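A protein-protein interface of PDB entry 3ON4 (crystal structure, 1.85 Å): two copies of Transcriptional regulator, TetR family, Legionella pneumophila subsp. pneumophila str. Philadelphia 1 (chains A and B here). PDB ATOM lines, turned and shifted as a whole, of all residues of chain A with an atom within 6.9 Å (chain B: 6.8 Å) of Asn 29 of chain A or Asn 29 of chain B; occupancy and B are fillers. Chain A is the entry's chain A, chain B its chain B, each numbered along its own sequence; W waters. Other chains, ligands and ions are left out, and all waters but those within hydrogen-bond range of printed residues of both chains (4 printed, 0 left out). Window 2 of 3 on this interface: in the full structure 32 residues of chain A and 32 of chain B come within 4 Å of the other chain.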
ATOM      1  N   ILE A  23      -7.647  26.940 -15.417  1.00  0.00           N
ATOM      2  CA  ILE A  23      -8.131  25.567 -15.260  1.00  0.00           C
ATOM      3  C   ILE A  23      -9.462  25.420 -15.995  1.00  0.00           C
ATOM      4  O   ILE A  23      -9.652  24.453 -16.772  1.00  0.00           O
ATOM      5  CB  ILE A  23      -8.245  25.140 -13.777  1.00  0.00           C
ATOM      6  CG1 ILE A  23      -6.837  25.047 -13.154  1.00  0.00           C
ATOM      7  CG2 ILE A  23      -9.000  23.793 -13.678  1.00  0.00           C
ATOM      8  CD1 ILE A  23      -6.852  24.968 -11.590  1.00  0.00           C
ATOM      9  N   ASP A  26      -8.533  25.584 -19.944  1.00  0.00           N
ATOM     10  CA  ASP A  26      -7.582  24.637 -20.562  1.00  0.00           C
ATOM     11  C   ASP A  26      -7.384  23.344 -19.816  1.00  0.00           C
ATOM     12  O   ASP A  26      -6.957  22.344 -20.424  1.00  0.00           O
ATOM     13  CB  ASP A  26      -6.199  25.280 -20.686  1.00  0.00           C
ATOM     14  CG  ASP A  26      -6.184  26.488 -21.595  1.00  0.00           C
ATOM     15  OD1 ASP A  26      -7.060  26.640 -22.482  1.00  0.00           O
ATOM     16  OD2 ASP A  26      -5.262  27.312 -21.415  1.00  0.00           O
ATOM     17  N   GLY A  27      -7.648  23.355 -18.511  1.00  0.00           N
ATOM     18  CA  GLY A  27      -7.520  22.158 -17.685  1.00  0.00           C
ATOM     19  C   GLY A  27      -6.252  22.182 -16.858  1.00  0.00           C
ATOM     20  O   GLY A  27      -5.272  22.796 -17.250  1.00  0.00           O
ATOM     21  N   TYR A  28      -6.289  21.497 -15.716  1.00  0.00           N
ATOM     22  CA  TYR A  28      -5.196  21.477 -14.738  1.00  0.00           C
ATOM     23  C   TYR A  28      -3.858  21.035 -15.299  1.00  0.00           C
ATOM     24  O   TYR A  28      -2.848  21.552 -14.901  1.00  0.00           O
ATOM     25  CB  TYR A  28      -5.584  20.542 -13.596  1.00  0.00           C
ATOM     26  CG  TYR A  28      -4.595  20.444 -12.448  1.00  0.00           C
ATOM     27  CD1 TYR A  28      -4.533  21.429 -11.462  1.00  0.00           C
ATOM     28  CD2 TYR A  28      -3.736  19.367 -12.335  1.00  0.00           C
ATOM     29  CE1 TYR A  28      -3.639  21.337 -10.402  1.00  0.00           C
ATOM     30  CE2 TYR A  28      -2.839  19.274 -11.279  1.00  0.00           C
ATOM     31  CZ  TYR A  28      -2.804  20.272 -10.312  1.00  0.00           C
ATOM     32  OH  TYR A  28      -1.916  20.158  -9.271  1.00  0.00           O
ATOM     33  N   ASN A  29      -3.849  20.053 -16.193  1.00  0.00           N
ATOM     34  CA  ASN A  29      -2.606  19.547 -16.786  1.00  0.00           C
ATOM     35  C   ASN A  29      -2.109  20.377 -17.997  1.00  0.00           C
ATOM     36  O   ASN A  29      -1.161  19.993 -18.690  1.00  0.00           O
ATOM     37  CB  ASN A  29      -2.775  18.080 -17.189  1.00  0.00           C
ATOM     38  CG  ASN A  29      -2.988  17.170 -15.987  1.00  0.00           C
ATOM     39  OD1 ASN A  29      -2.306  17.315 -14.961  1.00  0.00           O
ATOM     40  ND2 ASN A  29      -3.923  16.224 -16.109  1.00  0.00           N
ATOM     41  N   ALA A  30      -2.781  21.501 -18.248  1.00  0.00           N
ATOM     42  CA  ALA A  30      -2.437  22.380 -19.339  1.00  0.00           C
ATOM     43  C   ALA A  30      -2.168  23.816 -18.881  1.00  0.00           C
ATOM     44  O   ALA A  30      -2.284  24.747 -19.682  1.00  0.00           O
ATOM     45  CB  ALA A  30      -3.573  22.381 -20.358  1.00  0.00           C
ATOM     46  N   PHE A  31      -1.843  24.034 -17.611  1.00  0.00           N
ATOM     47  CA  PHE A  31      -1.289  25.321 -17.216  1.00  0.00           C
ATOM     48  C   PHE A  31      -0.141  25.070 -16.258  1.00  0.00           C
ATOM     49  O   PHE A  31      -0.022  23.983 -15.687  1.00  0.00           O
ATOM     50  CB  PHE A  31      -2.334  26.211 -16.554  1.00  0.00           C
ATOM     51  CG  PHE A  31      -2.485  25.950 -15.080  1.00  0.00           C
ATOM     52  CD1 PHE A  31      -3.224  24.876 -14.628  1.00  0.00           C
ATOM     53  CD2 PHE A  31      -1.837  26.759 -14.150  1.00  0.00           C
ATOM     54  CE1 PHE A  31      -3.336  24.598 -13.262  1.00  0.00           C
ATOM     55  CE2 PHE A  31      -1.925  26.479 -12.774  1.00  0.00           C
ATOM     56  CZ  PHE A  31      -2.689  25.411 -12.336  1.00  0.00           C
ATOM     57  N   SER A  32       0.691  26.081 -16.077  1.00  0.00           N
ATOM     58  CA  SER A  32       1.845  26.005 -15.190  1.00  0.00           C
ATOM     59  C   SER A  32       1.925  27.267 -14.334  1.00  0.00           C
ATOM     60  O   SER A  32       1.314  28.271 -14.645  1.00  0.00           O
ATOM     61  CB  SER A  32       3.127  25.875 -16.012  1.00  0.00           C
ATOM     62  OG  SER A  32       3.436  27.107 -16.646  1.00  0.00           O
ATOM     63  N   LYS A  54       2.234  22.561  -7.228  1.00  0.00           N
ATOM     64  CA  LYS A  54       1.020  22.754  -8.030  1.00  0.00           C
ATOM     65  C   LYS A  54      -0.192  22.166  -7.311  1.00  0.00           C
ATOM     66  O   LYS A  54      -1.268  22.767  -7.346  1.00  0.00           O
ATOM     67  CB  LYS A  54       1.171  22.126  -9.401  1.00  0.00           C
ATOM     68  CG  LYS A  54       0.122  22.515 -10.420  1.00  0.00           C
ATOM     69  CD  LYS A  54       0.451  21.855 -11.741  1.00  0.00           C
ATOM     70  CE  LYS A  54      -0.539  22.191 -12.795  1.00  0.00           C
ATOM     71  NZ  LYS A  54      -0.208  21.597 -14.133  1.00  0.00           N
ATOM     72  N   ASP A 115     -10.055  15.191 -15.568  1.00  0.00           N
ATOM     73  CA  ASP A 115      -8.645  14.935 -15.287  1.00  0.00           C
ATOM     74  C   ASP A 115      -8.425  13.999 -14.092  1.00  0.00           C
ATOM     75  O   ASP A 115      -7.277  13.699 -13.752  1.00  0.00           O
ATOM     76  CB  ASP A 115      -7.939  16.266 -14.984  1.00  0.00           C
ATOM     77  CG  ASP A 115      -7.990  17.236 -16.145  1.00  0.00           C
ATOM     78  OD1 ASP A 115      -7.980  16.778 -17.307  1.00  0.00           O
ATOM     79  OD2 ASP A 115      -8.064  18.452 -15.891  1.00  0.00           O
ATOM     80  N   PHE A 116      -9.523  13.522 -13.497  1.00  0.00           N
ATOM     81  CA  PHE A 116      -9.533  12.903 -12.146  1.00  0.00           C
ATOM     82  C   PHE A 116      -8.432  11.880 -11.898  1.00  0.00           C
ATOM     83  O   PHE A 116      -7.725  11.949 -10.876  1.00  0.00           O
ATOM     84  CB  PHE A 116     -10.914  12.299 -11.905  1.00  0.00           C
ATOM     85  CG  PHE A 116     -11.225  12.010 -10.473  1.00  0.00           C
ATOM     86  CD1 PHE A 116     -11.747  13.006  -9.658  1.00  0.00           C
ATOM     87  CD2 PHE A 116     -11.047  10.746  -9.955  1.00  0.00           C
ATOM     88  CE1 PHE A 116     -12.079  12.739  -8.352  1.00  0.00           C
ATOM     89  CE2 PHE A 116     -11.360  10.471  -8.630  1.00  0.00           C
ATOM     90  CZ  PHE A 116     -11.890  11.478  -7.837  1.00  0.00           C
ATOM     91  N   SER A 118      -5.582  11.534 -13.149  1.00  0.00           N
ATOM     92  CA  SER A 118      -4.237  12.091 -13.186  1.00  0.00           C
ATOM     93  C   SER A 118      -3.930  12.953 -11.949  1.00  0.00           C
ATOM     94  O   SER A 118      -2.780  13.384 -11.768  1.00  0.00           O
ATOM     95  CB  SER A 118      -4.043  12.948 -14.457  1.00  0.00           C
ATOM     96  OG  SER A 118      -4.682  14.221 -14.326  1.00  0.00           O
ATOM     97  N   LEU A 119      -4.941  13.206 -11.119  1.00  0.00           N
ATOM     98  CA  LEU A 119      -4.823  14.159 -10.010  1.00  0.00           C
ATOM     99  C   LEU A 119      -4.321  13.523  -8.715  1.00  0.00           C
ATOM    100  O   LEU A 119      -4.605  12.373  -8.432  1.00  0.00           O
ATOM    101  CB  LEU A 119      -6.176  14.812  -9.723  1.00  0.00           C
ATOM    102  CG  LEU A 119      -6.897  15.539 -10.859  1.00  0.00           C
ATOM    103  CD1 LEU A 119      -8.318  15.948 -10.432  1.00  0.00           C
ATOM    104  CD2 LEU A 119      -6.094  16.756 -11.308  1.00  0.00           C
ATOM    105  N   ILE B  23      -5.546   7.870 -22.863  1.00  0.00           N
ATOM    106  CA  ILE B  23      -6.338   9.079 -23.051  1.00  0.00           C
ATOM    107  C   ILE B  23      -7.695   8.930 -22.346  1.00  0.00           C
ATOM    108  O   ILE B  23      -8.132   9.829 -21.617  1.00  0.00           O
ATOM    109  CB  ILE B  23      -6.510   9.428 -24.554  1.00  0.00           C
ATOM    110  CG1 ILE B  23      -5.159   9.815 -25.200  1.00  0.00           C
ATOM    111  CG2 ILE B  23      -7.485  10.609 -24.720  1.00  0.00           C
ATOM    112  CD1 ILE B  23      -5.179   9.728 -26.691  1.00  0.00           C
ATOM    113  N   ASP B  26      -6.822   9.012 -18.376  1.00  0.00           N
ATOM    114  CA  ASP B  26      -6.118  10.174 -17.777  1.00  0.00           C
ATOM    115  C   ASP B  26      -6.203  11.477 -18.578  1.00  0.00           C
ATOM    116  O   ASP B  26      -5.995  12.539 -17.996  1.00  0.00           O
ATOM    117  CB  ASP B  26      -4.599   9.864 -17.581  1.00  0.00           C
ATOM    118  CG  ASP B  26      -4.331   8.639 -16.707  1.00  0.00           C
ATOM    119  OD1 ASP B  26      -5.177   8.245 -15.882  1.00  0.00           O
ATOM    120  OD2 ASP B  26      -3.233   8.053 -16.865  1.00  0.00           O
ATOM    121  N   GLY B  27      -6.435  11.391 -19.893  1.00  0.00           N
ATOM    122  CA  GLY B  27      -6.539  12.562 -20.767  1.00  0.00           C
ATOM    123  C   GLY B  27      -5.250  12.804 -21.549  1.00  0.00           C
ATOM    124  O   GLY B  27      -4.153  12.409 -21.130  1.00  0.00           O
ATOM    125  N   TYR B  28      -5.421  13.443 -22.693  1.00  0.00           N
ATOM    126  CA  TYR B  28      -4.349  13.658 -23.660  1.00  0.00           C
ATOM    127  C   TYR B  28      -3.134  14.361 -23.044  1.00  0.00           C
ATOM    128  O   TYR B  28      -2.005  14.040 -23.359  1.00  0.00           O
ATOM    129  CB  TYR B  28      -4.883  14.473 -24.798  1.00  0.00           C
ATOM    130  CG  TYR B  28      -3.885  14.754 -25.899  1.00  0.00           C
ATOM    131  CD1 TYR B  28      -3.625  13.808 -26.867  1.00  0.00           C
ATOM    132  CD2 TYR B  28      -3.257  16.000 -25.999  1.00  0.00           C
ATOM    133  CE1 TYR B  28      -2.740  14.091 -27.922  1.00  0.00           C
ATOM    134  CE2 TYR B  28      -2.360  16.283 -27.041  1.00  0.00           C
ATOM    135  CZ  TYR B  28      -2.120  15.320 -27.994  1.00  0.00           C
ATOM    136  OH  TYR B  28      -1.249  15.591 -29.030  1.00  0.00           O
ATOM    137  N   ASN B  29      -3.369  15.334 -22.170  1.00  0.00           N
ATOM    138  CA  ASN B  29      -2.267  16.095 -21.613  1.00  0.00           C
ATOM    139  C   ASN B  29      -1.625  15.421 -20.397  1.00  0.00           C
ATOM    140  O   ASN B  29      -0.744  16.002 -19.758  1.00  0.00           O
ATOM    141  CB  ASN B  29      -2.699  17.508 -21.223  1.00  0.00           C
ATOM    142  CG  ASN B  29      -3.085  18.340 -22.411  1.00  0.00           C
ATOM    143  OD1 ASN B  29      -2.374  18.353 -23.437  1.00  0.00           O
ATOM    144  ND2 ASN B  29      -4.192  19.061 -22.293  1.00  0.00           N
ATOM    145  N   ALA B  30      -2.058  14.202 -20.083  1.00  0.00           N
ATOM    146  CA  ALA B  30      -1.510  13.468 -18.957  1.00  0.00           C
ATOM    147  C   ALA B  30      -0.836  12.154 -19.361  1.00  0.00           C
ATOM    148  O   ALA B  30      -0.631  11.279 -18.507  1.00  0.00           O
ATOM    149  CB  ALA B  30      -2.628  13.189 -17.939  1.00  0.00           C
ATOM    150  N   PHE B  31      -0.533  11.982 -20.638  1.00  0.00           N
ATOM    151  CA  PHE B  31       0.306  10.867 -21.073  1.00  0.00           C
ATOM    152  C   PHE B  31       1.391  11.394 -22.018  1.00  0.00           C
ATOM    153  O   PHE B  31       1.244  12.460 -22.618  1.00  0.00           O
ATOM    154  CB  PHE B  31      -0.507   9.752 -21.736  1.00  0.00           C
ATOM    155  CG  PHE B  31      -0.699   9.935 -23.212  1.00  0.00           C
ATOM    156  CD1 PHE B  31      -1.672  10.789 -23.696  1.00  0.00           C
ATOM    157  CD2 PHE B  31       0.124   9.289 -24.127  1.00  0.00           C
ATOM    158  CE1 PHE B  31      -1.835  10.987 -25.051  1.00  0.00           C
ATOM    159  CE2 PHE B  31      -0.047   9.486 -25.496  1.00  0.00           C
ATOM    160  CZ  PHE B  31      -1.027  10.337 -25.952  1.00  0.00           C
ATOM    161  N   SER B  32       2.484  10.636 -22.117  1.00  0.00           N
ATOM    162  CA  SER B  32       3.585  10.926 -23.045  1.00  0.00           C
ATOM    163  C   SER B  32       3.932   9.660 -23.837  1.00  0.00           C
ATOM    164  O   SER B  32       3.478   8.542 -23.518  1.00  0.00           O
ATOM    165  CB  SER B  32       4.814  11.368 -22.260  1.00  0.00           C
ATOM    166  OG  SER B  32       5.335  10.280 -21.490  1.00  0.00           O
ATOM    167  N   LYS B  54       3.335  13.992 -31.105  1.00  0.00           N
ATOM    168  CA  LYS B  54       2.207  13.554 -30.300  1.00  0.00           C
ATOM    169  C   LYS B  54       0.880  13.904 -30.961  1.00  0.00           C
ATOM    170  O   LYS B  54      -0.033  13.105 -30.953  1.00  0.00           O
ATOM    171  CB  LYS B  54       2.268  14.206 -28.923  1.00  0.00           C
ATOM    172  CG  LYS B  54       1.389  13.557 -27.894  1.00  0.00           C
ATOM    173  CD  LYS B  54       1.362  14.443 -26.638  1.00  0.00           C
ATOM    174  CE  LYS B  54       0.483  13.885 -25.585  1.00  0.00           C
ATOM    175  NZ  LYS B  54       0.646  14.645 -24.315  1.00  0.00           N
ATOM    176  N   ASP B 115     -10.435  19.002 -22.916  1.00  0.00           N
ATOM    177  CA  ASP B 115      -9.098  19.501 -23.173  1.00  0.00           C
ATOM    178  C   ASP B 115      -9.028  20.469 -24.368  1.00  0.00           C
ATOM    179  O   ASP B 115      -7.969  21.028 -24.662  1.00  0.00           O
ATOM    180  CB  ASP B 115      -8.162  18.305 -23.462  1.00  0.00           C
ATOM    181  CG  ASP B 115      -8.000  17.363 -22.257  1.00  0.00           C
ATOM    182  OD1 ASP B 115      -8.031  17.867 -21.115  1.00  0.00           O
ATOM    183  OD2 ASP B 115      -7.822  16.139 -22.466  1.00  0.00           O
ATOM    184  N   PHE B 116     -10.157  20.684 -25.028  1.00  0.00           N
ATOM    185  CA  PHE B 116     -10.217  21.285 -26.371  1.00  0.00           C
ATOM    186  C   PHE B 116      -9.372  22.535 -26.584  1.00  0.00           C
ATOM    187  O   PHE B 116      -8.633  22.645 -27.568  1.00  0.00           O
ATOM    188  CB  PHE B 116     -11.678  21.621 -26.645  1.00  0.00           C
ATOM    189  CG  PHE B 116     -11.977  21.943 -28.043  1.00  0.00           C
ATOM    190  CD1 PHE B 116     -12.288  20.941 -28.943  1.00  0.00           C
ATOM    191  CD2 PHE B 116     -12.031  23.257 -28.457  1.00  0.00           C
ATOM    192  CE1 PHE B 116     -12.634  21.247 -30.253  1.00  0.00           C
ATOM    193  CE2 PHE B 116     -12.389  23.577 -29.762  1.00  0.00           C
ATOM    194  CZ  PHE B 116     -12.667  22.566 -30.668  1.00  0.00           C
ATOM    195  N   SER B 118      -6.726  23.525 -25.285  1.00  0.00           N
ATOM    196  CA  SER B 118      -5.314  23.258 -25.206  1.00  0.00           C
ATOM    197  C   SER B 118      -4.798  22.463 -26.402  1.00  0.00           C
ATOM    198  O   SER B 118      -3.596  22.269 -26.510  1.00  0.00           O
ATOM    199  CB  SER B 118      -4.998  22.474 -23.923  1.00  0.00           C
ATOM    200  OG  SER B 118      -5.407  21.132 -24.049  1.00  0.00           O
ATOM    201  N   LEU B 119      -5.687  22.029 -27.284  1.00  0.00           N
ATOM    202  CA  LEU B 119      -5.316  21.098 -28.368  1.00  0.00           C
ATOM    203  C   LEU B 119      -4.998  21.800 -29.677  1.00  0.00           C
ATOM    204  O   LEU B 119      -5.580  22.846 -30.004  1.00  0.00           O
ATOM    205  CB  LEU B 119      -6.435  20.099 -28.650  1.00  0.00           C
ATOM    206  CG  LEU B 119      -7.012  19.237 -27.521  1.00  0.00           C
ATOM    207  CD1 LEU B 119      -8.305  18.579 -27.993  1.00  0.00           C
ATOM    208  CD2 LEU B 119      -6.025  18.184 -27.079  1.00  0.00           C
HETATM  209  O   HOH W   1      -8.873  15.005 -20.018  1.00  0.00           O
HETATM  210  O   HOH W   2      -5.829  15.289 -18.020  1.00  0.00           O
HETATM  211  O   HOH W   3      -9.380  19.358 -18.412  1.00  0.00           O
HETATM  212  O   HOH W   4      -6.232  19.699 -20.453  1.00  0.00           O
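The backbone carbonyl oxygen of Asp 115 of chain B sits at hydrogen-bond distance from the side-chain hydroxyl of Ser 118 of chain B.
The side-chain amide nitrogen (ND2) of Asn 29 of chain A sits at hydrogen-bond distance from the side-chain hydroxyl (OG) of Ser 118 of chain A (2.8 Å).
The side-chain hydroxyl of Ser 118 of chain A is in hydrogen-bond range of the backbone carbonyl oxygen of Asp 115 of chain A (2.7 Å).
OG of Ser 118 of chain B sits at hydrogen-bond distance from ND2 of Asn 29 of chain B (3.0 Å).
O of Asn 29 of chain A touches CB of Asn 29 of chain B, at 3.9 Å.
Ala 30 of chain B touches Asn 29 of chain A.
Ala 30 of chain A touches Asn 29 of chain B (CB to ND2, 3.9 Å).
Ala 30 of chain A touches Ser 118 of chain B (CB to CB, 3.8 Å).
OD1 of Asp 115 of chain A touches OD1 of Asp 115 of chain B, 3.96 Å away.
CB of Ala 30 of chain B touches CB of Ser 118 of chain A, 3.8 Å away.
Asn 29 of chain A touches just these residues of chain B: Asn 29 and Ala 30.
Phe 31 of chain A touches none of the printed residues of chain B.
Printed residues of chain A within 4 Å of Ala 30 of chain B: Asn 29 and Ser 118.
Of the printed residues of chain A, Ser 118 of chain B touches Ala 30 (3.8 Å).
The nearest residue of chain A that does not touch Asn 29 of chain B is Asp 26 of chain A (4.7 Å).
The nearest printed residue of chain B that does not touch Asp 115 of chain A is Asp 26 of chain B (4.5 Å).
Printed residues of chain A that touch a printed residue of chain B: Asn 29, Ala 30, Asp 115 and Ser 118.
Hydrophobic or aromatic side chains of chain A that line the printed part of chain B: Ala 30.
Of the 13 printed residues of chain B, 4 touch a printed residue of chain A.
Printed residues of chain B that touch a printed residue of chain A: Asn 29, Ala 30, Asp 115 and Ser 118.
Hydrophobic or aromatic side chains of chain B that line the printed part of chain A: Ala 30.
Along chain B the printed residues that touch a printed residue of chain A span positions 29 to 118.
Among the printed residues, no Asp or Glu carboxylate lies within 4 Å of a Lys or Arg side-chain nitrogen of the other chain.
Asn 29 of chain A touches its own counterpart, Asn 29 of chain B.
Asn 29 of chain A touches Ala 30 of chain B, and with the chains exchanged Ala 30 of chain A touches Asn 29 of chain B.
Ala 30 of chain A touches Ser 118 of chain B, and with the chains exchanged Ser 118 of chain A touches Ala 30 of chain B.
Asp 115 of chain A touches its own counterpart, Asp 115 of chain B.
Positions printed for both chains: 23, 26, 27, 28, 29, 30, 31, 32, 54, 115, 116, 118 and 119.
Of the 6 pairs that touch across the chains among the printed residues, 6 have their exchanged pair printed and touching as well.
Water W4 lies within hydrogen-bond range of OD1 of Asp 115 of chain B (2.7 Å), O of Asp 26 of chain A (2.7 Å) and ND2 of Asn 29 of chain B (2.8 Å).
Water W2 lies within hydrogen-bond range of OD1 of Asp 115 of chain A, O of Asp 26 of chain B and ND2 of Asn 29 of chain A.
Water W1 lies within hydrogen-bond range of the side-chain carboxylate (OD2) of Asp 115 of chain B (2.9 Å) and the side-chain carboxylate (OD1) of Asp 115 of chain A (3.4 Å).
Water W3 lies within hydrogen-bond range of OD2 of Asp 115 of chain A (3.0 Å) and OD1 of Asp 115 of chain B (3.4 Å).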
